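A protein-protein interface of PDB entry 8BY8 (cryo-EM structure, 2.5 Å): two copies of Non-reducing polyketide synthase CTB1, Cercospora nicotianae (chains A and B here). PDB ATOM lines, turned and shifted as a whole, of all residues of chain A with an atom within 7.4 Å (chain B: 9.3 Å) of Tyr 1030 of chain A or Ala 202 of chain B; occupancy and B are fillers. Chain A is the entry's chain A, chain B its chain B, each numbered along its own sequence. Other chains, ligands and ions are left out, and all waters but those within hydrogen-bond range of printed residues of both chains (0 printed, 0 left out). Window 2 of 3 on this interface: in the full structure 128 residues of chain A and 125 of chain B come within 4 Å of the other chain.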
ATOM      1  N   ILE A 954     -15.619 -18.151   3.626  1.00  0.00           N
ATOM      2  CA  ILE A 954     -16.115 -19.238   4.464  1.00  0.00           C
ATOM      3  C   ILE A 954     -17.626 -19.136   4.625  1.00  0.00           C
ATOM      4  O   ILE A 954     -18.359 -20.111   4.422  1.00  0.00           O
ATOM      5  CB  ILE A 954     -15.400 -19.232   5.827  1.00  0.00           C
ATOM      6  CG1 ILE A 954     -14.005 -19.838   5.685  1.00  0.00           C
ATOM      7  CG2 ILE A 954     -16.220 -19.990   6.860  1.00  0.00           C
ATOM      8  CD1 ILE A 954     -13.094 -19.596   6.868  1.00  0.00           C
ATOM      9  N   CYS A 955     -18.117 -17.947   4.982  1.00  0.00           N
ATOM     10  CA  CYS A 955     -19.543 -17.773   5.231  1.00  0.00           C
ATOM     11  C   CYS A 955     -20.356 -18.067   3.979  1.00  0.00           C
ATOM     12  O   CYS A 955     -21.388 -18.742   4.041  1.00  0.00           O
ATOM     13  CB  CYS A 955     -19.813 -16.354   5.734  1.00  0.00           C
ATOM     14  SG  CYS A 955     -19.110 -15.993   7.362  1.00  0.00           S
ATOM     15  N   MET A 958     -20.899 -21.808   3.451  1.00  0.00           N
ATOM     16  CA  MET A 958     -21.905 -22.471   4.274  1.00  0.00           C
ATOM     17  C   MET A 958     -23.252 -21.755   4.237  1.00  0.00           C
ATOM     18  O   MET A 958     -23.987 -21.761   5.228  1.00  0.00           O
ATOM     19  CB  MET A 958     -21.407 -22.597   5.716  1.00  0.00           C
ATOM     20  CG  MET A 958     -20.922 -21.298   6.334  1.00  0.00           C
ATOM     21  SD  MET A 958     -20.421 -21.466   8.055  1.00  0.00           S
ATOM     22  CE  MET A 958     -19.144 -22.712   7.930  1.00  0.00           C
ATOM     23  N   LEU A 960     -24.355 -18.436   3.999  1.00  0.00           N
ATOM     24  CA  LEU A 960     -24.551 -17.292   4.871  1.00  0.00           C
ATOM     25  C   LEU A 960     -24.357 -16.013   4.070  1.00  0.00           C
ATOM     26  O   LEU A 960     -23.632 -16.008   3.071  1.00  0.00           O
ATOM     27  CB  LEU A 960     -23.571 -17.316   6.054  1.00  0.00           C
ATOM     28  CG  LEU A 960     -23.712 -18.476   7.042  1.00  0.00           C
ATOM     29  CD1 LEU A 960     -22.645 -18.385   8.120  1.00  0.00           C
ATOM     30  CD2 LEU A 960     -25.095 -18.499   7.670  1.00  0.00           C
ATOM     31  N   LEU A 983     -23.308 -11.609  12.212  1.00  0.00           N
ATOM     32  CA  LEU A 983     -22.146 -12.138  11.510  1.00  0.00           C
ATOM     33  C   LEU A 983     -21.069 -11.072  11.372  1.00  0.00           C
ATOM     34  O   LEU A 983     -19.883 -11.341  11.599  1.00  0.00           O
ATOM     35  CB  LEU A 983     -22.554 -12.667  10.133  1.00  0.00           C
ATOM     36  CG  LEU A 983     -23.127 -14.084  10.068  1.00  0.00           C
ATOM     37  CD1 LEU A 983     -23.675 -14.373   8.684  1.00  0.00           C
ATOM     38  CD2 LEU A 983     -22.077 -15.113  10.435  1.00  0.00           C
ATOM     39  N   TYR A1014     -18.556 -15.835  22.021  1.00  0.00           N
ATOM     40  CA  TYR A1014     -18.089 -16.622  20.885  1.00  0.00           C
ATOM     41  C   TYR A1014     -16.684 -16.203  20.465  1.00  0.00           C
ATOM     42  O   TYR A1014     -15.772 -17.036  20.376  1.00  0.00           O
ATOM     43  CB  TYR A1014     -19.070 -16.472  19.722  1.00  0.00           C
ATOM     44  CG  TYR A1014     -20.346 -17.263  19.887  1.00  0.00           C
ATOM     45  CD1 TYR A1014     -21.380 -16.796  20.688  1.00  0.00           C
ATOM     46  CD2 TYR A1014     -20.520 -18.475  19.235  1.00  0.00           C
ATOM     47  CE1 TYR A1014     -22.551 -17.517  20.835  1.00  0.00           C
ATOM     48  CE2 TYR A1014     -21.687 -19.203  19.376  1.00  0.00           C
ATOM     49  CZ  TYR A1014     -22.696 -18.720  20.177  1.00  0.00           C
ATOM     50  OH  TYR A1014     -23.859 -19.443  20.318  1.00  0.00           O
ATOM     51  N   SER A1024     -12.597 -22.852  16.655  1.00  0.00           N
ATOM     52  CA  SER A1024     -11.898 -22.301  15.509  1.00  0.00           C
ATOM     53  C   SER A1024     -12.706 -21.147  14.922  1.00  0.00           C
ATOM     54  O   SER A1024     -13.842 -20.885  15.318  1.00  0.00           O
ATOM     55  CB  SER A1024     -11.658 -23.380  14.453  1.00  0.00           C
ATOM     56  OG  SER A1024     -12.879 -23.840  13.903  1.00  0.00           O
ATOM     57  N   GLN A1025     -12.100 -20.446  13.963  1.00  0.00           N
ATOM     58  CA  GLN A1025     -12.807 -19.363  13.290  1.00  0.00           C
ATOM     59  C   GLN A1025     -14.046 -19.886  12.578  1.00  0.00           C
ATOM     60  O   GLN A1025     -15.144 -19.330  12.717  1.00  0.00           O
ATOM     61  CB  GLN A1025     -11.873 -18.669  12.299  1.00  0.00           C
ATOM     62  CG  GLN A1025     -10.587 -18.151  12.923  1.00  0.00           C
ATOM     63  CD  GLN A1025      -9.639 -17.546  11.908  1.00  0.00           C
ATOM     64  OE1 GLN A1025      -9.141 -16.438  12.095  1.00  0.00           O
ATOM     65  NE2 GLN A1025      -9.372 -18.279  10.833  1.00  0.00           N
ATOM     66  N   SER A1026     -13.892 -20.972  11.816  1.00  0.00           N
ATOM     67  CA  SER A1026     -15.018 -21.511  11.064  1.00  0.00           C
ATOM     68  C   SER A1026     -16.118 -22.003  11.995  1.00  0.00           C
ATOM     69  O   SER A1026     -17.307 -21.811  11.716  1.00  0.00           O
ATOM     70  CB  SER A1026     -14.543 -22.639  10.150  1.00  0.00           C
ATOM     71  OG  SER A1026     -15.619 -23.166   9.396  1.00  0.00           O
ATOM     72  N   ASP A1027     -15.744 -22.645  13.104  1.00  0.00           N
ATOM     73  CA  ASP A1027     -16.744 -23.119  14.056  1.00  0.00           C
ATOM     74  C   ASP A1027     -17.532 -21.955  14.638  1.00  0.00           C
ATOM     75  O   ASP A1027     -18.762 -22.012  14.744  1.00  0.00           O
ATOM     76  CB  ASP A1027     -16.073 -23.922  15.173  1.00  0.00           C
ATOM     77  CG  ASP A1027     -15.662 -25.316  14.731  1.00  0.00           C
ATOM     78  OD1 ASP A1027     -16.310 -25.866  13.816  1.00  0.00           O
ATOM     79  OD2 ASP A1027     -14.697 -25.863  15.307  1.00  0.00           O
ATOM     80  N   THR A1028     -16.835 -20.887  15.027  1.00  0.00           N
ATOM     81  CA  THR A1028     -17.509 -19.720  15.586  1.00  0.00           C
ATOM     82  C   THR A1028     -18.465 -19.106  14.571  1.00  0.00           C
ATOM     83  O   THR A1028     -19.622 -18.798  14.890  1.00  0.00           O
ATOM     84  CB  THR A1028     -16.469 -18.693  16.036  1.00  0.00           C
ATOM     85  OG1 THR A1028     -15.427 -19.347  16.770  1.00  0.00           O
ATOM     86  CG2 THR A1028     -17.102 -17.646  16.920  1.00  0.00           C
ATOM     87  N   LEU A1029     -17.997 -18.925  13.332  1.00  0.00           N
ATOM     88  CA  LEU A1029     -18.855 -18.341  12.309  1.00  0.00           C
ATOM     89  C   LEU A1029     -20.082 -19.207  12.064  1.00  0.00           C
ATOM     90  O   LEU A1029     -21.205 -18.698  11.992  1.00  0.00           O
ATOM     91  CB  LEU A1029     -18.072 -18.150  11.009  1.00  0.00           C
ATOM     92  CG  LEU A1029     -16.883 -17.190  11.075  1.00  0.00           C
ATOM     93  CD1 LEU A1029     -16.097 -17.231   9.775  1.00  0.00           C
ATOM     94  CD2 LEU A1029     -17.335 -15.772  11.387  1.00  0.00           C
ATOM     95  N   TYR A1030     -19.888 -20.522  11.942  1.00  0.00           N
ATOM     96  CA  TYR A1030     -21.009 -21.416  11.680  1.00  0.00           C
ATOM     97  C   TYR A1030     -22.010 -21.392  12.827  1.00  0.00           C
ATOM     98  O   TYR A1030     -23.225 -21.338  12.601  1.00  0.00           O
ATOM     99  CB  TYR A1030     -20.487 -22.833  11.446  1.00  0.00           C
ATOM    100  CG  TYR A1030     -21.557 -23.866  11.189  1.00  0.00           C
ATOM    101  CD1 TYR A1030     -22.258 -23.887   9.992  1.00  0.00           C
ATOM    102  CD2 TYR A1030     -21.851 -24.837  12.136  1.00  0.00           C
ATOM    103  CE1 TYR A1030     -23.230 -24.835   9.750  1.00  0.00           C
ATOM    104  CE2 TYR A1030     -22.820 -25.789  11.904  1.00  0.00           C
ATOM    105  CZ  TYR A1030     -23.506 -25.783  10.710  1.00  0.00           C
ATOM    106  OH  TYR A1030     -24.473 -26.732  10.475  1.00  0.00           O
ATOM    107  N   LEU A1031     -21.519 -21.415  14.066  1.00  0.00           N
ATOM    108  CA  LEU A1031     -22.412 -21.433  15.216  1.00  0.00           C
ATOM    109  C   LEU A1031     -23.231 -20.150  15.289  1.00  0.00           C
ATOM    110  O   LEU A1031     -24.457 -20.191  15.460  1.00  0.00           O
ATOM    111  CB  LEU A1031     -21.592 -21.637  16.490  1.00  0.00           C
ATOM    112  CG  LEU A1031     -22.206 -22.402  17.664  1.00  0.00           C
ATOM    113  CD1 LEU A1031     -22.937 -23.652  17.208  1.00  0.00           C
ATOM    114  CD2 LEU A1031     -21.108 -22.767  18.644  1.00  0.00           C
ATOM    115  N   VAL A1032     -22.571 -18.997  15.147  1.00  0.00           N
ATOM    116  CA  VAL A1032     -23.291 -17.727  15.210  1.00  0.00           C
ATOM    117  C   VAL A1032     -24.295 -17.624  14.070  1.00  0.00           C
ATOM    118  O   VAL A1032     -25.446 -17.208  14.270  1.00  0.00           O
ATOM    119  CB  VAL A1032     -22.300 -16.549  15.201  1.00  0.00           C
ATOM    120  CG1 VAL A1032     -23.045 -15.232  15.046  1.00  0.00           C
ATOM    121  CG2 VAL A1032     -21.471 -16.547  16.476  1.00  0.00           C
ATOM    122  N   GLY A1033     -23.883 -17.992  12.855  1.00  0.00           N
ATOM    123  CA  GLY A1033     -24.787 -17.898  11.725  1.00  0.00           C
ATOM    124  C   GLY A1033     -25.999 -18.794  11.874  1.00  0.00           C
ATOM    125  O   GLY A1033     -27.118 -18.401  11.539  1.00  0.00           O
ATOM    126  N   ARG A1034     -25.799 -20.011  12.386  1.00  0.00           N
ATOM    127  CA  ARG A1034     -26.923 -20.925  12.557  1.00  0.00           C
ATOM    128  C   ARG A1034     -27.854 -20.454  13.667  1.00  0.00           C
ATOM    129  O   ARG A1034     -29.079 -20.574  13.545  1.00  0.00           O
ATOM    130  CB  ARG A1034     -26.406 -22.334  12.838  1.00  0.00           C
ATOM    131  CG  ARG A1034     -25.652 -22.942  11.668  1.00  0.00           C
ATOM    132  CD  ARG A1034     -26.425 -24.083  11.023  1.00  0.00           C
ATOM    133  NE  ARG A1034     -27.758 -23.686  10.587  1.00  0.00           N
ATOM    134  CZ  ARG A1034     -28.045 -23.191   9.390  1.00  0.00           C
ATOM    135  NH1 ARG A1034     -27.107 -22.995   8.478  1.00  0.00           N
ATOM    136  NH2 ARG A1034     -29.306 -22.886   9.100  1.00  0.00           N
ATOM    137  N   ARG A1035     -27.302 -19.907  14.755  1.00  0.00           N
ATOM    138  CA  ARG A1035     -28.164 -19.362  15.799  1.00  0.00           C
ATOM    139  C   ARG A1035     -29.006 -18.212  15.262  1.00  0.00           C
ATOM    140  O   ARG A1035     -30.212 -18.132  15.533  1.00  0.00           O
ATOM    141  CB  ARG A1035     -27.330 -18.897  16.993  1.00  0.00           C
ATOM    142  CG  ARG A1035     -28.170 -18.529  18.202  1.00  0.00           C
ATOM    143  CD  ARG A1035     -27.325 -18.114  19.395  1.00  0.00           C
ATOM    144  NE  ARG A1035     -27.019 -16.688  19.392  1.00  0.00           N
ATOM    145  CZ  ARG A1035     -26.639 -16.001  20.461  1.00  0.00           C
ATOM    146  NH1 ARG A1035     -26.512 -16.577  21.646  1.00  0.00           N
ATOM    147  NH2 ARG A1035     -26.387 -14.702  20.342  1.00  0.00           N
ATOM    148  N   ALA A1036     -28.387 -17.314  14.491  1.00  0.00           N
ATOM    149  CA  ALA A1036     -29.138 -16.211  13.903  1.00  0.00           C
ATOM    150  C   ALA A1036     -30.190 -16.719  12.924  1.00  0.00           C
ATOM    151  O   ALA A1036     -31.302 -16.183  12.864  1.00  0.00           O
ATOM    152  CB  ALA A1036     -28.186 -15.241  13.208  1.00  0.00           C
ATOM    153  N   GLN A1037     -29.853 -17.746  12.141  1.00  0.00           N
ATOM    154  CA  GLN A1037     -30.824 -18.316  11.214  1.00  0.00           C
ATOM    155  C   GLN A1037     -32.029 -18.875  11.957  1.00  0.00           C
ATOM    156  O   GLN A1037     -33.175 -18.657  11.548  1.00  0.00           O
ATOM    157  CB  GLN A1037     -30.162 -19.410  10.378  1.00  0.00           C
ATOM    158  CG  GLN A1037     -29.193 -18.896   9.329  1.00  0.00           C
ATOM    159  CD  GLN A1037     -29.875 -18.606   8.009  1.00  0.00           C
ATOM    160  OE1 GLN A1037     -31.035 -18.196   7.974  1.00  0.00           O
ATOM    161  NE2 GLN A1037     -29.160 -18.829   6.912  1.00  0.00           N
ATOM    162  N   GLN A1129     -28.316 -29.315  18.688  1.00  0.00           N
ATOM    163  CA  GLN A1129     -27.789 -30.207  17.663  1.00  0.00           C
ATOM    164  C   GLN A1129     -26.634 -29.546  16.924  1.00  0.00           C
ATOM    165  O   GLN A1129     -25.564 -30.142  16.753  1.00  0.00           O
ATOM    166  CB  GLN A1129     -28.914 -30.606  16.705  1.00  0.00           C
ATOM    167  CG  GLN A1129     -28.454 -31.201  15.386  1.00  0.00           C
ATOM    168  CD  GLN A1129     -28.502 -30.193  14.253  1.00  0.00           C
ATOM    169  OE1 GLN A1129     -29.492 -29.480  14.088  1.00  0.00           O
ATOM    170  NE2 GLN A1129     -27.433 -30.126  13.470  1.00  0.00           N
ATOM    171  N   VAL A1130     -26.816 -28.288  16.515  1.00  0.00           N
ATOM    172  CA  VAL A1130     -25.743 -27.580  15.824  1.00  0.00           C
ATOM    173  C   VAL A1130     -24.523 -27.468  16.727  1.00  0.00           C
ATOM    174  O   VAL A1130     -23.383 -27.640  16.280  1.00  0.00           O
ATOM    175  CB  VAL A1130     -26.232 -26.198  15.351  1.00  0.00           C
ATOM    176  CG1 VAL A1130     -25.087 -25.401  14.750  1.00  0.00           C
ATOM    177  CG2 VAL A1130     -27.361 -26.359  14.346  1.00  0.00           C
ATOM    178  N   ALA A1131     -24.739 -27.190  18.013  1.00  0.00           N
ATOM    179  CA  ALA A1131     -23.618 -27.079  18.935  1.00  0.00           C
ATOM    180  C   ALA A1131     -22.853 -28.387  19.065  1.00  0.00           C
ATOM    181  O   ALA A1131     -21.691 -28.375  19.484  1.00  0.00           O
ATOM    182  CB  ALA A1131     -24.112 -26.620  20.306  1.00  0.00           C
ATOM    183  N   ALA A1133     -22.131 -30.268  16.440  1.00  0.00           N
ATOM    184  CA  ALA A1133     -21.303 -30.401  15.246  1.00  0.00           C
ATOM    185  C   ALA A1133     -19.895 -29.867  15.481  1.00  0.00           C
ATOM    186  O   ALA A1133     -18.917 -30.436  14.983  1.00  0.00           O
ATOM    187  CB  ALA A1133     -21.961 -29.676  14.072  1.00  0.00           C
ATOM    188  N   CYS A1134     -19.772 -28.776  16.232  1.00  0.00           N
ATOM    189  CA  CYS A1134     -18.476 -28.152  16.441  1.00  0.00           C
ATOM    190  C   CYS A1134     -17.516 -29.120  17.132  1.00  0.00           C
ATOM    191  O   CYS A1134     -17.902 -30.179  17.632  1.00  0.00           O
ATOM    192  CB  CYS A1134     -18.627 -26.879  17.272  1.00  0.00           C
ATOM    193  SG  CYS A1134     -19.771 -25.674  16.564  1.00  0.00           S
ATOM    194  N   LEU B 162      -9.672 -23.576   9.216  1.00  0.00           N
ATOM    195  CA  LEU B 162     -10.677 -24.621   9.376  1.00  0.00           C
ATOM    196  C   LEU B 162     -10.492 -25.457  10.638  1.00  0.00           C
ATOM    197  O   LEU B 162     -11.420 -26.182  11.015  1.00  0.00           O
ATOM    198  CB  LEU B 162     -10.659 -25.540   8.154  1.00  0.00           C
ATOM    199  CG  LEU B 162     -12.006 -25.950   7.561  1.00  0.00           C
ATOM    200  CD1 LEU B 162     -12.819 -24.733   7.150  1.00  0.00           C
ATOM    201  CD2 LEU B 162     -11.781 -26.869   6.373  1.00  0.00           C
ATOM    202  N   THR B 196     -21.881 -38.076   6.672  1.00  0.00           N
ATOM    203  CA  THR B 196     -22.222 -36.662   6.775  1.00  0.00           C
ATOM    204  C   THR B 196     -23.687 -36.476   7.148  1.00  0.00           C
ATOM    205  O   THR B 196     -24.016 -35.645   8.002  1.00  0.00           O
ATOM    206  CB  THR B 196     -21.918 -35.956   5.454  1.00  0.00           C
ATOM    207  OG1 THR B 196     -20.571 -36.236   5.059  1.00  0.00           O
ATOM    208  CG2 THR B 196     -22.104 -34.451   5.596  1.00  0.00           C
ATOM    209  N   GLN B 199     -24.114 -37.682  10.899  1.00  0.00           N
ATOM    210  CA  GLN B 199     -23.459 -36.736  11.786  1.00  0.00           C
ATOM    211  C   GLN B 199     -23.930 -35.315  11.485  1.00  0.00           C
ATOM    212  O   GLN B 199     -24.517 -35.031  10.438  1.00  0.00           O
ATOM    213  CB  GLN B 199     -21.941 -36.837  11.635  1.00  0.00           C
ATOM    214  CG  GLN B 199     -21.152 -36.416  12.864  1.00  0.00           C
ATOM    215  CD  GLN B 199     -21.029 -37.528  13.884  1.00  0.00           C
ATOM    216  OE1 GLN B 199     -21.751 -38.523  13.825  1.00  0.00           O
ATOM    217  NE2 GLN B 199     -20.106 -37.369  14.825  1.00  0.00           N
ATOM    218  N   ALA B 200     -23.670 -34.412  12.427  1.00  0.00           N
ATOM    219  CA  ALA B 200     -23.904 -32.984  12.237  1.00  0.00           C
ATOM    220  C   ALA B 200     -22.558 -32.326  11.954  1.00  0.00           C
ATOM    221  O   ALA B 200     -21.694 -32.265  12.834  1.00  0.00           O
ATOM    222  CB  ALA B 200     -24.571 -32.367  13.464  1.00  0.00           C
ATOM    223  N   LEU B 201     -22.378 -31.845  10.725  1.00  0.00           N
ATOM    224  CA  LEU B 201     -21.112 -31.272  10.294  1.00  0.00           C
ATOM    225  C   LEU B 201     -21.357 -30.017   9.472  1.00  0.00           C
ATOM    226  O   LEU B 201     -22.286 -29.967   8.662  1.00  0.00           O
ATOM    227  CB  LEU B 201     -20.302 -32.275   9.462  1.00  0.00           C
ATOM    228  CG  LEU B 201     -19.626 -33.412  10.228  1.00  0.00           C
ATOM    229  CD1 LEU B 201     -19.079 -34.447   9.263  1.00  0.00           C
ATOM    230  CD2 LEU B 201     -18.520 -32.872  11.116  1.00  0.00           C
ATOM    231  N   ALA B 202     -20.519 -29.006   9.687  1.00  0.00           N
ATOM    232  CA  ALA B 202     -20.531 -27.836   8.824  1.00  0.00           C
ATOM    233  C   ALA B 202     -20.079 -28.222   7.422  1.00  0.00           C
ATOM    234  O   ALA B 202     -19.231 -29.101   7.246  1.00  0.00           O
ATOM    235  CB  ALA B 202     -19.621 -26.746   9.391  1.00  0.00           C
ATOM    236  N   SER B 203     -20.649 -27.558   6.415  1.00  0.00           N
ATOM    237  CA  SER B 203     -20.339 -27.910   5.034  1.00  0.00           C
ATOM    238  C   SER B 203     -18.871 -27.689   4.695  1.00  0.00           C
ATOM    239  O   SER B 203     -18.389 -28.241   3.699  1.00  0.00           O
ATOM    240  CB  SER B 203     -21.218 -27.103   4.079  1.00  0.00           C
ATOM    241  OG  SER B 203     -21.174 -27.646   2.771  1.00  0.00           O
ATOM    242  N   VAL B 204     -18.149 -26.901   5.494  1.00  0.00           N
ATOM    243  CA  VAL B 204     -16.731 -26.644   5.261  1.00  0.00           C
ATOM    244  C   VAL B 204     -15.844 -27.542   6.116  1.00  0.00           C
ATOM    245  O   VAL B 204     -14.624 -27.355   6.142  1.00  0.00           O
ATOM    246  CB  VAL B 204     -16.391 -25.164   5.500  1.00  0.00           C
ATOM    247  CG1 VAL B 204     -17.298 -24.265   4.674  1.00  0.00           C
ATOM    248  CG2 VAL B 204     -16.488 -24.822   6.980  1.00  0.00           C
ATOM    249  N   SER B 205     -16.426 -28.514   6.820  1.00  0.00           N
ATOM    250  CA  SER B 205     -15.662 -29.432   7.651  1.00  0.00           C
ATOM    251  C   SER B 205     -15.924 -30.895   7.324  1.00  0.00           C
ATOM    252  O   SER B 205     -15.356 -31.769   7.986  1.00  0.00           O
ATOM    253  CB  SER B 205     -15.964 -29.184   9.136  1.00  0.00           C
ATOM    254  OG  SER B 205     -15.300 -28.023   9.599  1.00  0.00           O
ATOM    255  N   VAL B 206     -16.749 -31.184   6.327  1.00  0.00           N
ATOM    256  CA  VAL B 206     -17.073 -32.577   6.001  1.00  0.00           C
ATOM    257  C   VAL B 206     -15.882 -33.220   5.303  1.00  0.00           C
ATOM    258  O   VAL B 206     -15.212 -32.552   4.494  1.00  0.00           O
ATOM    259  CB  VAL B 206     -18.325 -32.632   5.123  1.00  0.00           C
ATOM    260  CG1 VAL B 206     -18.038 -32.047   3.747  1.00  0.00           C
ATOM    261  CG2 VAL B 206     -18.835 -34.055   5.009  1.00  0.00           C
ATOM    262  N   PRO B 207     -15.566 -34.489   5.574  1.00  0.00           N
ATOM    263  CA  PRO B 207     -14.517 -35.160   4.798  1.00  0.00           C
ATOM    264  C   PRO B 207     -14.901 -35.281   3.332  1.00  0.00           C
ATOM    265  O   PRO B 207     -16.078 -35.394   2.981  1.00  0.00           O
ATOM    266  CB  PRO B 207     -14.404 -36.537   5.463  1.00  0.00           C
ATOM    267  CG  PRO B 207     -14.927 -36.343   6.832  1.00  0.00           C
ATOM    268  CD  PRO B 207     -16.010 -35.314   6.712  1.00  0.00           C
ATOM    269  N   ILE B 226     -11.656 -34.829  12.529  1.00  0.00           N
ATOM    270  CA  ILE B 226     -12.760 -35.378  11.750  1.00  0.00           C
ATOM    271  C   ILE B 226     -12.293 -36.585  10.950  1.00  0.00           C
ATOM    272  O   ILE B 226     -13.021 -37.574  10.809  1.00  0.00           O
ATOM    273  CB  ILE B 226     -13.365 -34.291  10.844  1.00  0.00           C
ATOM    274  CG1 ILE B 226     -13.789 -33.089  11.689  1.00  0.00           C
ATOM    275  CG2 ILE B 226     -14.560 -34.835  10.068  1.00  0.00           C
ATOM    276  CD1 ILE B 226     -14.427 -31.983  10.898  1.00  0.00           C
ATOM    277  N   HIS B 253     -14.775 -27.148  -2.351  1.00  0.00           N
ATOM    278  CA  HIS B 253     -15.667 -26.482  -1.413  1.00  0.00           C
ATOM    279  C   HIS B 253     -14.915 -25.592  -0.433  1.00  0.00           C
ATOM    280  O   HIS B 253     -15.530 -25.040   0.486  1.00  0.00           O
ATOM    281  CB  HIS B 253     -16.493 -27.520  -0.651  1.00  0.00           C
ATOM    282  CG  HIS B 253     -15.666 -28.543   0.060  1.00  0.00           C
ATOM    283  ND1 HIS B 253     -15.114 -28.323   1.302  1.00  0.00           N
ATOM    284  CD2 HIS B 253     -15.286 -29.791  -0.305  1.00  0.00           C
ATOM    285  CE1 HIS B 253     -14.434 -29.392   1.676  1.00  0.00           C
ATOM    286  NE2 HIS B 253     -14.523 -30.297   0.718  1.00  0.00           N
ATOM    287  N   LEU B 254     -13.600 -25.441  -0.602  1.00  0.00           N
ATOM    288  CA  LEU B 254     -12.805 -24.569   0.245  1.00  0.00           C
ATOM    289  C   LEU B 254     -12.002 -23.533  -0.525  1.00  0.00           C
ATOM    290  O   LEU B 254     -11.465 -22.611   0.098  1.00  0.00           O
ATOM    291  CB  LEU B 254     -11.832 -25.395   1.103  1.00  0.00           C
ATOM    292  CG  LEU B 254     -12.433 -26.359   2.126  1.00  0.00           C
ATOM    293  CD1 LEU B 254     -11.325 -27.020   2.931  1.00  0.00           C
ATOM    294  CD2 LEU B 254     -13.406 -25.644   3.048  1.00  0.00           C
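Of the 25 printed residues of chain A, 6 touch a printed residue of chain B. Hydrophobic or aromatic side chains of chain A that line the printed part of chain B: Met 958, Tyr 1030 and Ala 1133. Hydrophobic or aromatic side chains of chain B that line the printed part of chain A: Leu 162, Ala 200, Ala 202 and Val 204. Among the printed residues, no Asp or Glu carboxylate lies within 4 Å of a Lys or Arg side-chain nitrogen of the other chain.
The side-chain hydroxyl of Ser 1024 of chain A sits at hydrogen-bond distance from the side-chain carboxylate of Asp 1027 of chain A. The side-chain hydroxyl (OG1) of Thr 1028 of chain A lies within hydrogen-bond range of the backbone carbonyl oxygen (O) of Ser 1024 of chain A (2.6 Å).
No position is printed for both chains.
Of the printed residues of chain B, Tyr 1030 of chain A touches Ala 202 (3.9 Å). Ala 202 of chain B touches one residue of chain A. Of the printed residues of chain B, Met 958 of chain A touches Val 204. Of the printed residues of chain A, Val 204 of chain B touches Met 958 and Ser 1026. Printed residues of chain B within 4 Å of Ser 1026 of chain A: Leu 162 and Val 204. Of the printed residues of chain B, Ser 1024 of chain A touches Leu 162. The nearest residue of chain A that does not touch Ala 202 of chain B is Met 958 of chain A (4.3 Å). The nearest printed residue of chain A that does not touch Val 204 of chain B is Ile 954 of chain A (4.3 Å).
Among the printed residues, pairs that only touch across the chains: Ala 1133 of chain A with Ala 200 of chain B (2.9 Å), Ser 1026 of chain A with Val 204 of chain B (3.1 Å), Met 958 of chain A with Val 204 of chain B (3.5 Å), Gln 1129 of chain A with Ala 200 of chain B (3.6 Å), Tyr 1030 of chain A with Ala 202 of chain B (3.9 Å), Ser 1026 of chain A with Leu 162 of chain B (3.9 Å) and Ser 1024 of chain A with Leu 162 of chain B (3.99 Å).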
